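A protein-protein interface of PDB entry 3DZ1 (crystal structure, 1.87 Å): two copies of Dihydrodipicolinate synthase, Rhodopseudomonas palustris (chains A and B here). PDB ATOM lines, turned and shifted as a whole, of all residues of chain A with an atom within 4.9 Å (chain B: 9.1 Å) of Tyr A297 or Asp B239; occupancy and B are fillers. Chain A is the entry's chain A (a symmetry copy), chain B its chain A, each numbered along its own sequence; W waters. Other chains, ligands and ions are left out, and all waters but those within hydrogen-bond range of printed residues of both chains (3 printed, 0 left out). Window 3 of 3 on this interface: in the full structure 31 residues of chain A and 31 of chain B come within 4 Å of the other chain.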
ATOM      1  N   GLU A 293       5.315  21.183   6.799  1.00  0.00           N
ATOM      2  CA  GLU A 293       6.083  21.622   5.635  1.00  0.00           C
ATOM      3  C   GLU A 293       5.130  22.016   4.506  1.00  0.00           C
ATOM      4  O   GLU A 293       5.329  23.031   3.837  1.00  0.00           O
ATOM      5  CB  GLU A 293       7.012  20.500   5.152  1.00  0.00           C
ATOM      6  CG  GLU A 293       8.015  20.906   4.067  1.00  0.00           C
ATOM      7  CD  GLU A 293       7.370  21.220   2.728  1.00  0.00           C
ATOM      8  OE1 GLU A 293       6.409  20.521   2.357  1.00  0.00           O
ATOM      9  OE2 GLU A 293       7.833  22.152   2.033  1.00  0.00           O
ATOM     10  N   GLU A 294       4.099  21.205   4.296  1.00  0.00           N
ATOM     11  CA  GLU A 294       3.126  21.482   3.243  1.00  0.00           C
ATOM     12  C   GLU A 294       2.428  22.813   3.504  1.00  0.00           C
ATOM     13  O   GLU A 294       2.222  23.599   2.582  1.00  0.00           O
ATOM     14  CB  GLU A 294       2.105  20.343   3.149  1.00  0.00           C
ATOM     15  CG  GLU A 294       2.753  18.984   2.880  1.00  0.00           C
ATOM     16  CD  GLU A 294       1.763  17.839   2.871  1.00  0.00           C
ATOM     17  OE1 GLU A 294       0.854  17.834   3.723  1.00  0.00           O
ATOM     18  OE2 GLU A 294       1.905  16.933   2.022  1.00  0.00           O
ATOM     19  N   VAL A 295       2.062  23.061   4.759  1.00  0.00           N
ATOM     20  CA  VAL A 295       1.416  24.320   5.117  1.00  0.00           C
ATOM     21  C   VAL A 295       2.413  25.452   4.867  1.00  0.00           C
ATOM     22  O   VAL A 295       2.053  26.498   4.329  1.00  0.00           O
ATOM     23  CB  VAL A 295       0.987  24.343   6.604  1.00  0.00           C
ATOM     24  CG1 VAL A 295       0.500  25.747   6.990  1.00  0.00           C
ATOM     25  CG2 VAL A 295      -0.118  23.316   6.837  1.00  0.00           C
ATOM     26  N   ASP A 296       3.665  25.238   5.264  1.00  0.00           N
ATOM     27  CA  ASP A 296       4.705  26.243   5.059  1.00  0.00           C
ATOM     28  C   ASP A 296       4.850  26.556   3.575  1.00  0.00           C
ATOM     29  O   ASP A 296       5.053  27.708   3.190  1.00  0.00           O
ATOM     30  CB  ASP A 296       6.059  25.758   5.592  1.00  0.00           C
ATOM     31  CG  ASP A 296       6.113  25.705   7.108  1.00  0.00           C
ATOM     32  OD1 ASP A 296       5.233  26.305   7.758  1.00  0.00           O
ATOM     33  OD2 ASP A 296       7.048  25.071   7.649  1.00  0.00           O
ATOM     34  N   TYR A 297       4.759  25.524   2.741  1.00  0.00           N
ATOM     35  CA  TYR A 297       4.885  25.709   1.298  1.00  0.00           C
ATOM     36  C   TYR A 297       3.770  26.620   0.786  1.00  0.00           C
ATOM     37  O   TYR A 297       4.019  27.553   0.020  1.00  0.00           O
ATOM     38  CB  TYR A 297       4.822  24.360   0.576  1.00  0.00           C
ATOM     39  CG  TYR A 297       5.011  24.463  -0.921  1.00  0.00           C
ATOM     40  CD1 TYR A 297       6.221  24.893  -1.465  1.00  0.00           C
ATOM     41  CD2 TYR A 297       3.979  24.134  -1.797  1.00  0.00           C
ATOM     42  CE1 TYR A 297       6.398  24.991  -2.850  1.00  0.00           C
ATOM     43  CE2 TYR A 297       4.145  24.225  -3.181  1.00  0.00           C
ATOM     44  CZ  TYR A 297       5.355  24.653  -3.700  1.00  0.00           C
ATOM     45  OH  TYR A 297       5.516  24.731  -5.065  1.00  0.00           O
ATOM     46  N   LEU A 298       2.542  26.346   1.209  1.00  0.00           N
ATOM     47  CA  LEU A 298       1.404  27.153   0.789  1.00  0.00           C
ATOM     48  C   LEU A 298       1.581  28.594   1.261  1.00  0.00           C
ATOM     49  O   LEU A 298       1.295  29.539   0.521  1.00  0.00           O
ATOM     50  CB  LEU A 298       0.105  26.571   1.350  1.00  0.00           C
ATOM     51  CG  LEU A 298      -0.283  25.181   0.831  1.00  0.00           C
ATOM     52  CD1 LEU A 298      -1.582  24.737   1.483  1.00  0.00           C
ATOM     53  CD2 LEU A 298      -0.426  25.213  -0.686  1.00  0.00           C
ATOM     54  N   LEU A 299       2.053  28.753   2.492  1.00  0.00           N
ATOM     55  CA  LEU A 299       2.283  30.076   3.060  1.00  0.00           C
ATOM     56  C   LEU A 299       3.311  30.854   2.246  1.00  0.00           C
ATOM     57  O   LEU A 299       3.154  32.058   2.018  1.00  0.00           O
ATOM     58  CB  LEU A 299       2.772  29.954   4.510  1.00  0.00           C
ATOM     59  CG  LEU A 299       1.744  29.514   5.557  1.00  0.00           C
ATOM     60  CD1 LEU A 299       2.435  29.242   6.899  1.00  0.00           C
ATOM     61  CD2 LEU A 299       0.682  30.599   5.710  1.00  0.00           C
ATOM     62  N   SER A 300       4.357  30.159   1.805  1.00  0.00           N
ATOM     63  CA  SER A 300       5.428  30.781   1.033  1.00  0.00           C
ATOM     64  C   SER A 300       4.951  31.275  -0.324  1.00  0.00           C
ATOM     65  O   SER A 300       5.489  32.248  -0.860  1.00  0.00           O
ATOM     66  CB  SER A 300       6.586  29.798   0.837  1.00  0.00           C
ATOM     67  OG  SER A 300       6.248  28.780  -0.088  1.00  0.00           O
ATOM     68  N   ARG A 301       3.947  30.604  -0.879  1.00  0.00           N
ATOM     69  CA  ARG A 301       3.406  30.978  -2.183  1.00  0.00           C
ATOM     70  C   ARG A 301       2.408  32.124  -2.082  1.00  0.00           C
ATOM     71  O   ARG A 301       2.133  32.810  -3.066  1.00  0.00           O
ATOM     72  CB  ARG A 301       2.759  29.760  -2.847  1.00  0.00           C
ATOM     73  CG  ARG A 301       3.781  28.721  -3.298  1.00  0.00           C
ATOM     74  CD  ARG A 301       3.148  27.377  -3.587  1.00  0.00           C
ATOM     75  NE  ARG A 301       2.211  27.411  -4.704  1.00  0.00           N
ATOM     76  CZ  ARG A 301       2.559  27.588  -5.973  1.00  0.00           C
ATOM     77  NH1 ARG A 301       3.833  27.752  -6.301  1.00  0.00           N
ATOM     78  NH2 ARG A 301       1.627  27.591  -6.916  1.00  0.00           N
ATOM     79  N   ASP B 206      -2.546  17.831  -5.532  1.00  0.00           N
ATOM     80  CA  ASP B 206      -1.219  18.422  -5.497  1.00  0.00           C
ATOM     81  C   ASP B 206      -0.333  17.786  -4.435  1.00  0.00           C
ATOM     82  O   ASP B 206       0.801  17.392  -4.719  1.00  0.00           O
ATOM     83  CB  ASP B 206      -1.314  19.947  -5.306  1.00  0.00           C
ATOM     84  CG  ASP B 206      -2.048  20.353  -4.039  1.00  0.00           C
ATOM     85  OD1 ASP B 206      -2.904  19.592  -3.541  1.00  0.00           O
ATOM     86  OD2 ASP B 206      -1.780  21.468  -3.545  1.00  0.00           O
ATOM     87  N   PHE B 207      -0.851  17.651  -3.221  1.00  0.00           N
ATOM     88  CA  PHE B 207      -0.069  17.059  -2.146  1.00  0.00           C
ATOM     89  C   PHE B 207      -0.135  15.537  -2.136  1.00  0.00           C
ATOM     90  O   PHE B 207       0.782  14.877  -1.658  1.00  0.00           O
ATOM     91  CB  PHE B 207      -0.513  17.638  -0.799  1.00  0.00           C
ATOM     92  CG  PHE B 207      -0.066  19.060  -0.583  1.00  0.00           C
ATOM     93  CD1 PHE B 207       1.290  19.367  -0.478  1.00  0.00           C
ATOM     94  CD2 PHE B 207      -0.991  20.097  -0.512  1.00  0.00           C
ATOM     95  CE1 PHE B 207       1.716  20.683  -0.308  1.00  0.00           C
ATOM     96  CE2 PHE B 207      -0.575  21.417  -0.341  1.00  0.00           C
ATOM     97  CZ  PHE B 207       0.782  21.709  -0.239  1.00  0.00           C
ATOM     98  N   GLU B 210       2.726  14.249  -3.910  1.00  0.00           N
ATOM     99  CA  GLU B 210       3.943  14.381  -3.114  1.00  0.00           C
ATOM    100  C   GLU B 210       4.042  13.277  -2.057  1.00  0.00           C
ATOM    101  O   GLU B 210       5.138  12.803  -1.736  1.00  0.00           O
ATOM    102  CB  GLU B 210       3.991  15.761  -2.445  1.00  0.00           C
ATOM    103  CG  GLU B 210       3.959  16.917  -3.442  1.00  0.00           C
ATOM    104  CD  GLU B 210       4.176  18.275  -2.798  1.00  0.00           C
ATOM    105  OE1 GLU B 210       4.260  18.345  -1.553  1.00  0.00           O
ATOM    106  OE2 GLU B 210       4.258  19.275  -3.544  1.00  0.00           O
ATOM    107  N   LEU B 232       3.900  16.662 -14.003  1.00  0.00           N
ATOM    108  CA  LEU B 232       4.786  17.628 -13.369  1.00  0.00           C
ATOM    109  C   LEU B 232       5.164  17.178 -11.970  1.00  0.00           C
ATOM    110  O   LEU B 232       6.310  17.350 -11.543  1.00  0.00           O
ATOM    111  CB  LEU B 232       4.122  19.006 -13.309  1.00  0.00           C
ATOM    112  CG  LEU B 232       3.968  19.735 -14.646  1.00  0.00           C
ATOM    113  CD1 LEU B 232       3.045  20.939 -14.477  1.00  0.00           C
ATOM    114  CD2 LEU B 232       5.347  20.163 -15.158  1.00  0.00           C
ATOM    115  N   SER B 233       4.204  16.597 -11.255  1.00  0.00           N
ATOM    116  CA  SER B 233       4.453  16.131  -9.899  1.00  0.00           C
ATOM    117  C   SER B 233       5.486  15.006  -9.894  1.00  0.00           C
ATOM    118  O   SER B 233       6.412  15.011  -9.078  1.00  0.00           O
ATOM    119  CB  SER B 233       3.153  15.646  -9.257  1.00  0.00           C
ATOM    120  OG  SER B 233       2.192  16.688  -9.206  1.00  0.00           O
ATOM    121  N   ALA B 235       7.698  14.515 -12.028  1.00  0.00           N
ATOM    122  CA  ALA B 235       8.966  15.078 -12.483  1.00  0.00           C
ATOM    123  C   ALA B 235       9.657  15.918 -11.408  1.00  0.00           C
ATOM    124  O   ALA B 235      10.733  16.474 -11.642  1.00  0.00           O
ATOM    125  CB  ALA B 235       8.739  15.918 -13.731  1.00  0.00           C
ATOM    126  N   GLY B 236       9.043  16.017 -10.235  1.00  0.00           N
ATOM    127  CA  GLY B 236       9.644  16.790  -9.164  1.00  0.00           C
ATOM    128  C   GLY B 236       9.586  18.297  -9.365  1.00  0.00           C
ATOM    129  O   GLY B 236      10.229  19.049  -8.632  1.00  0.00           O
ATOM    130  N   GLN B 237       8.826  18.737 -10.362  1.00  0.00           N
ATOM    131  CA  GLN B 237       8.673  20.158 -10.647  1.00  0.00           C
ATOM    132  C   GLN B 237       7.562  20.695  -9.749  1.00  0.00           C
ATOM    133  O   GLN B 237       6.465  21.011 -10.219  1.00  0.00           O
ATOM    134  CB  GLN B 237       8.299  20.361 -12.116  1.00  0.00           C
ATOM    135  CG  GLN B 237       9.427  20.087 -13.101  1.00  0.00           C
ATOM    136  CD  GLN B 237      10.628  20.996 -12.869  1.00  0.00           C
ATOM    137  OE1 GLN B 237      10.476  22.153 -12.477  1.00  0.00           O
ATOM    138  NE2 GLN B 237      11.824  20.481 -13.125  1.00  0.00           N
ATOM    139  N   ARG B 238       7.862  20.802  -8.457  1.00  0.00           N
ATOM    140  CA  ARG B 238       6.895  21.255  -7.465  1.00  0.00           C
ATOM    141  C   ARG B 238       6.171  22.564  -7.774  1.00  0.00           C
ATOM    142  O   ARG B 238       4.943  22.620  -7.721  1.00  0.00           O
ATOM    143  CB  ARG B 238       7.559  21.366  -6.086  1.00  0.00           C
ATOM    144  CG  ARG B 238       6.553  21.259  -4.939  1.00  0.00           C
ATOM    145  CD  ARG B 238       7.185  21.458  -3.566  1.00  0.00           C
ATOM    146  NE  ARG B 238       6.272  21.034  -2.506  1.00  0.00           N
ATOM    147  CZ  ARG B 238       6.466  21.252  -1.209  1.00  0.00           C
ATOM    148  NH1 ARG B 238       7.545  21.900  -0.793  1.00  0.00           N
ATOM    149  NH2 ARG B 238       5.582  20.808  -0.322  1.00  0.00           N
ATOM    150  N   ASP B 239       6.921  23.617  -8.082  1.00  0.00           N
ATOM    151  CA  ASP B 239       6.295  24.903  -8.368  1.00  0.00           C
ATOM    152  C   ASP B 239       5.406  24.850  -9.598  1.00  0.00           C
ATOM    153  O   ASP B 239       4.304  25.383  -9.583  1.00  0.00           O
ATOM    154  CB  ASP B 239       7.348  26.005  -8.536  1.00  0.00           C
ATOM    155  CG  ASP B 239       8.089  26.309  -7.241  1.00  0.00           C
ATOM    156  OD1 ASP B 239       7.578  25.948  -6.161  1.00  0.00           O
ATOM    157  OD2 ASP B 239       9.180  26.922  -7.299  1.00  0.00           O
ATOM    158  N   LEU B 240       5.877  24.213 -10.665  1.00  0.00           N
ATOM    159  CA  LEU B 240       5.080  24.121 -11.884  1.00  0.00           C
ATOM    160  C   LEU B 240       3.808  23.322 -11.630  1.00  0.00           C
ATOM    161  O   LEU B 240       2.724  23.699 -12.083  1.00  0.00           O
ATOM    162  CB  LEU B 240       5.883  23.461 -13.012  1.00  0.00           C
ATOM    163  CG  LEU B 240       7.116  24.232 -13.489  1.00  0.00           C
ATOM    164  CD1 LEU B 240       7.756  23.500 -14.660  1.00  0.00           C
ATOM    165  CD2 LEU B 240       6.711  25.633 -13.902  1.00  0.00           C
ATOM    166  N   ALA B 241       3.950  22.218 -10.908  1.00  0.00           N
ATOM    167  CA  ALA B 241       2.814  21.367 -10.590  1.00  0.00           C
ATOM    168  C   ALA B 241       1.780  22.146  -9.784  1.00  0.00           C
ATOM    169  O   ALA B 241       0.595  22.144 -10.119  1.00  0.00           O
ATOM    170  CB  ALA B 241       3.277  20.143  -9.809  1.00  0.00           C
ATOM    171  N   HIS B 242       2.224  22.808  -8.721  1.00  0.00           N
ATOM    172  CA  HIS B 242       1.311  23.590  -7.890  1.00  0.00           C
ATOM    173  C   HIS B 242       0.743  24.820  -8.598  1.00  0.00           C
ATOM    174  O   HIS B 242      -0.373  25.248  -8.303  1.00  0.00           O
ATOM    175  CB  HIS B 242       2.005  24.001  -6.590  1.00  0.00           C
ATOM    176  CG  HIS B 242       2.059  22.906  -5.573  1.00  0.00           C
ATOM    177  ND1 HIS B 242       1.107  22.762  -4.588  1.00  0.00           N
ATOM    178  CD2 HIS B 242       2.919  21.871  -5.423  1.00  0.00           C
ATOM    179  CE1 HIS B 242       1.378  21.684  -3.873  1.00  0.00           C
ATOM    180  NE2 HIS B 242       2.472  21.126  -4.360  1.00  0.00           N
ATOM    181  N   ASN B 243       1.497  25.403  -9.525  1.00  0.00           N
ATOM    182  CA  ASN B 243       0.977  26.565 -10.234  1.00  0.00           C
ATOM    183  C   ASN B 243      -0.215  26.158 -11.091  1.00  0.00           C
ATOM    184  O   ASN B 243      -1.246  26.837 -11.108  1.00  0.00           O
ATOM    185  CB  ASN B 243       2.050  27.197 -11.125  1.00  0.00           C
ATOM    186  CG  ASN B 243       3.101  27.949 -10.333  1.00  0.00           C
ATOM    187  OD1 ASN B 243       2.919  28.237  -9.145  1.00  0.00           O
ATOM    188  ND2 ASN B 243       4.206  28.284 -10.992  1.00  0.00           N
ATOM    189  N   LEU B 244      -0.071  25.044 -11.798  1.00  0.00           N
ATOM    190  CA  LEU B 244      -1.134  24.541 -12.660  1.00  0.00           C
ATOM    191  C   LEU B 244      -2.321  24.073 -11.833  1.00  0.00           C
ATOM    192  O   LEU B 244      -3.473  24.350 -12.172  1.00  0.00           O
ATOM    193  CB  LEU B 244      -0.615  23.390 -13.527  1.00  0.00           C
ATOM    194  CG  LEU B 244      -1.631  22.741 -14.472  1.00  0.00           C
ATOM    195  CD1 LEU B 244      -2.236  23.798 -15.391  1.00  0.00           C
ATOM    196  CD2 LEU B 244      -0.943  21.646 -15.281  1.00  0.00           C
ATOM    197  N   PHE B 245      -2.043  23.365 -10.742  1.00  0.00           N
ATOM    198  CA  PHE B 245      -3.114  22.891  -9.881  1.00  0.00           C
ATOM    199  C   PHE B 245      -3.900  24.090  -9.342  1.00  0.00           C
ATOM    200  O   PHE B 245      -5.126  24.131  -9.431  1.00  0.00           O
ATOM    201  CB  PHE B 245      -2.545  22.072  -8.712  1.00  0.00           C
ATOM    202  CG  PHE B 245      -3.596  21.539  -7.783  1.00  0.00           C
ATOM    203  CD1 PHE B 245      -4.337  20.407  -8.118  1.00  0.00           C
ATOM    204  CD2 PHE B 245      -3.870  22.188  -6.582  1.00  0.00           C
ATOM    205  CE1 PHE B 245      -5.336  19.929  -7.268  1.00  0.00           C
ATOM    206  CE2 PHE B 245      -4.866  21.720  -5.726  1.00  0.00           C
ATOM    207  CZ  PHE B 245      -5.600  20.587  -6.071  1.00  0.00           C
ATOM    208  N   ASP B 246      -3.184  25.071  -8.799  1.00  0.00           N
ATOM    209  CA  ASP B 246      -3.813  26.265  -8.230  1.00  0.00           C
ATOM    210  C   ASP B 246      -4.686  27.026  -9.215  1.00  0.00           C
ATOM    211  O   ASP B 246      -5.665  27.673  -8.817  1.00  0.00           O
ATOM    212  CB  ASP B 246      -2.750  27.217  -7.673  1.00  0.00           C
ATOM    213  CG  ASP B 246      -2.105  26.691  -6.409  1.00  0.00           C
ATOM    214  OD1 ASP B 246      -2.519  25.614  -5.923  1.00  0.00           O
ATOM    215  OD2 ASP B 246      -1.186  27.361  -5.897  1.00  0.00           O
ATOM    216  N   ALA B 247      -4.321  26.973 -10.492  1.00  0.00           N
ATOM    217  CA  ALA B 247      -5.086  27.648 -11.526  1.00  0.00           C
ATOM    218  C   ALA B 247      -6.415  26.924 -11.712  1.00  0.00           C
ATOM    219  O   ALA B 247      -7.426  27.533 -12.057  1.00  0.00           O
ATOM    220  CB  ALA B 247      -4.299  27.670 -12.840  1.00  0.00           C
HETATM  221  O   HOH W   1       4.403  16.789   0.833  1.00  0.00           O
HETATM  222  O   HOH W   2       6.547  28.313  -5.059  1.00  0.00           O
HETATM  223  O   HOH W   3      -0.294  27.002  -3.500  1.00  0.00           O
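Water W3 bridges OD2 of Asp B246 and NE of Arg A301. Water W1 bridges the side-chain carboxylate (OE2) of Glu A294 (2.8 Å) and the side-chain carboxylate (OE1) of Glu B210 (2.9 Å). Water W2 bridges the side-chain carboxylate (OD1) of Asp B239 (2.8 Å) and the guanidinium group (NH1) of Arg A301 (3.0 Å).
OD2 of Asp B206 lies close to ND1 of His B242 (3.3 Å). OE2 of Glu B210 lies within salt-bridge range of NE of Arg B238 (2.9 Å). The side-chain carboxylate (OE2) of Glu B210 is in hydrogen-bond range of a ring nitrogen (NE2) of His B242, at 2.7 Å. The side-chain amide oxygen (OD1) of Asn B243 sits close to the backbone carbonyl oxygen (O) of Asp B239. O of Tyr A297 lies within hydrogen-bond range of OG of Ser A300 (2.5 Å).
NH2 of Arg B238 is in salt-bridge range of OE1 of Glu A293 (2.8 Å). The backbone carbonyl oxygen (O) of Arg B238 sits at hydrogen-bond distance from the side-chain hydroxyl (OH) of Tyr A297 (3.4 Å). OD1 of Asp B239 is in hydrogen-bond range of OH of Tyr A297, at 2.6 Å. O of His B242 lies close to NH2 of Arg A301 (3.4 Å). The side-chain amide oxygen of Asn B243 is in hydrogen-bond range of the guanidinium group of Arg A301. The side-chain carboxylate (OD2) of Asp B246 lies within salt-bridge range of the guanidinium group (NH2) of Arg A301, 3.0 Å away.
No position is printed for both chains. Of the 9 pairs that touch across the chains among the printed residues, none has its exchanged pair printed and touching as well.
Hydrophobic or aromatic side chains of chain A that line the printed part of chain B: Tyr A297 and Leu A298. Of the 18 printed residues of chain B, 6 touch a printed residue of chain A. Among the printed residues, 9 pairs touch across the chains. Among the printed residues, Asp or Glu carboxylates within 4 Å of a Lys or Arg side-chain nitrogen of the other chain: Glu A293 with Arg B238 (2.8 Å) and Arg A301 with Asp B246 (3.0 Å).
Printed residues of chain B within 4 Å of Glu A293: Arg B238 (2.8 Å). Tyr A297 touches three residues of chain B. No residue of chain B comes within 4 Å of Ser A300. Of the printed residues of chain B, Arg A301 touches His B242, Asn B243 and Asp B246. Asp B206 touches none of the printed residues of chain A. Printed residues of chain A within 4 Å of Phe B207: Glu A294 (3.5 Å) and Leu A298 (3.7 Å). Leu B232 touches none of the printed residues of chain A. Of chain A, only Tyr A297 (2.6 Å) comes within 4 Å of Asp B239. Printed residues of chain A within 4 Å of Asn B243: Arg A301 (2.7 Å). Printed residues of chain A within 4 Å of Asp B246: Arg A301. The nearest printed residue of chain A that does not touch Asn B243 is Tyr A297 (6.0 Å).
Among the printed residues, pairs that only touch across the chains: Tyr A297 with His B242, Glu A294 with Phe B207 and Leu A298 with Phe B207.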
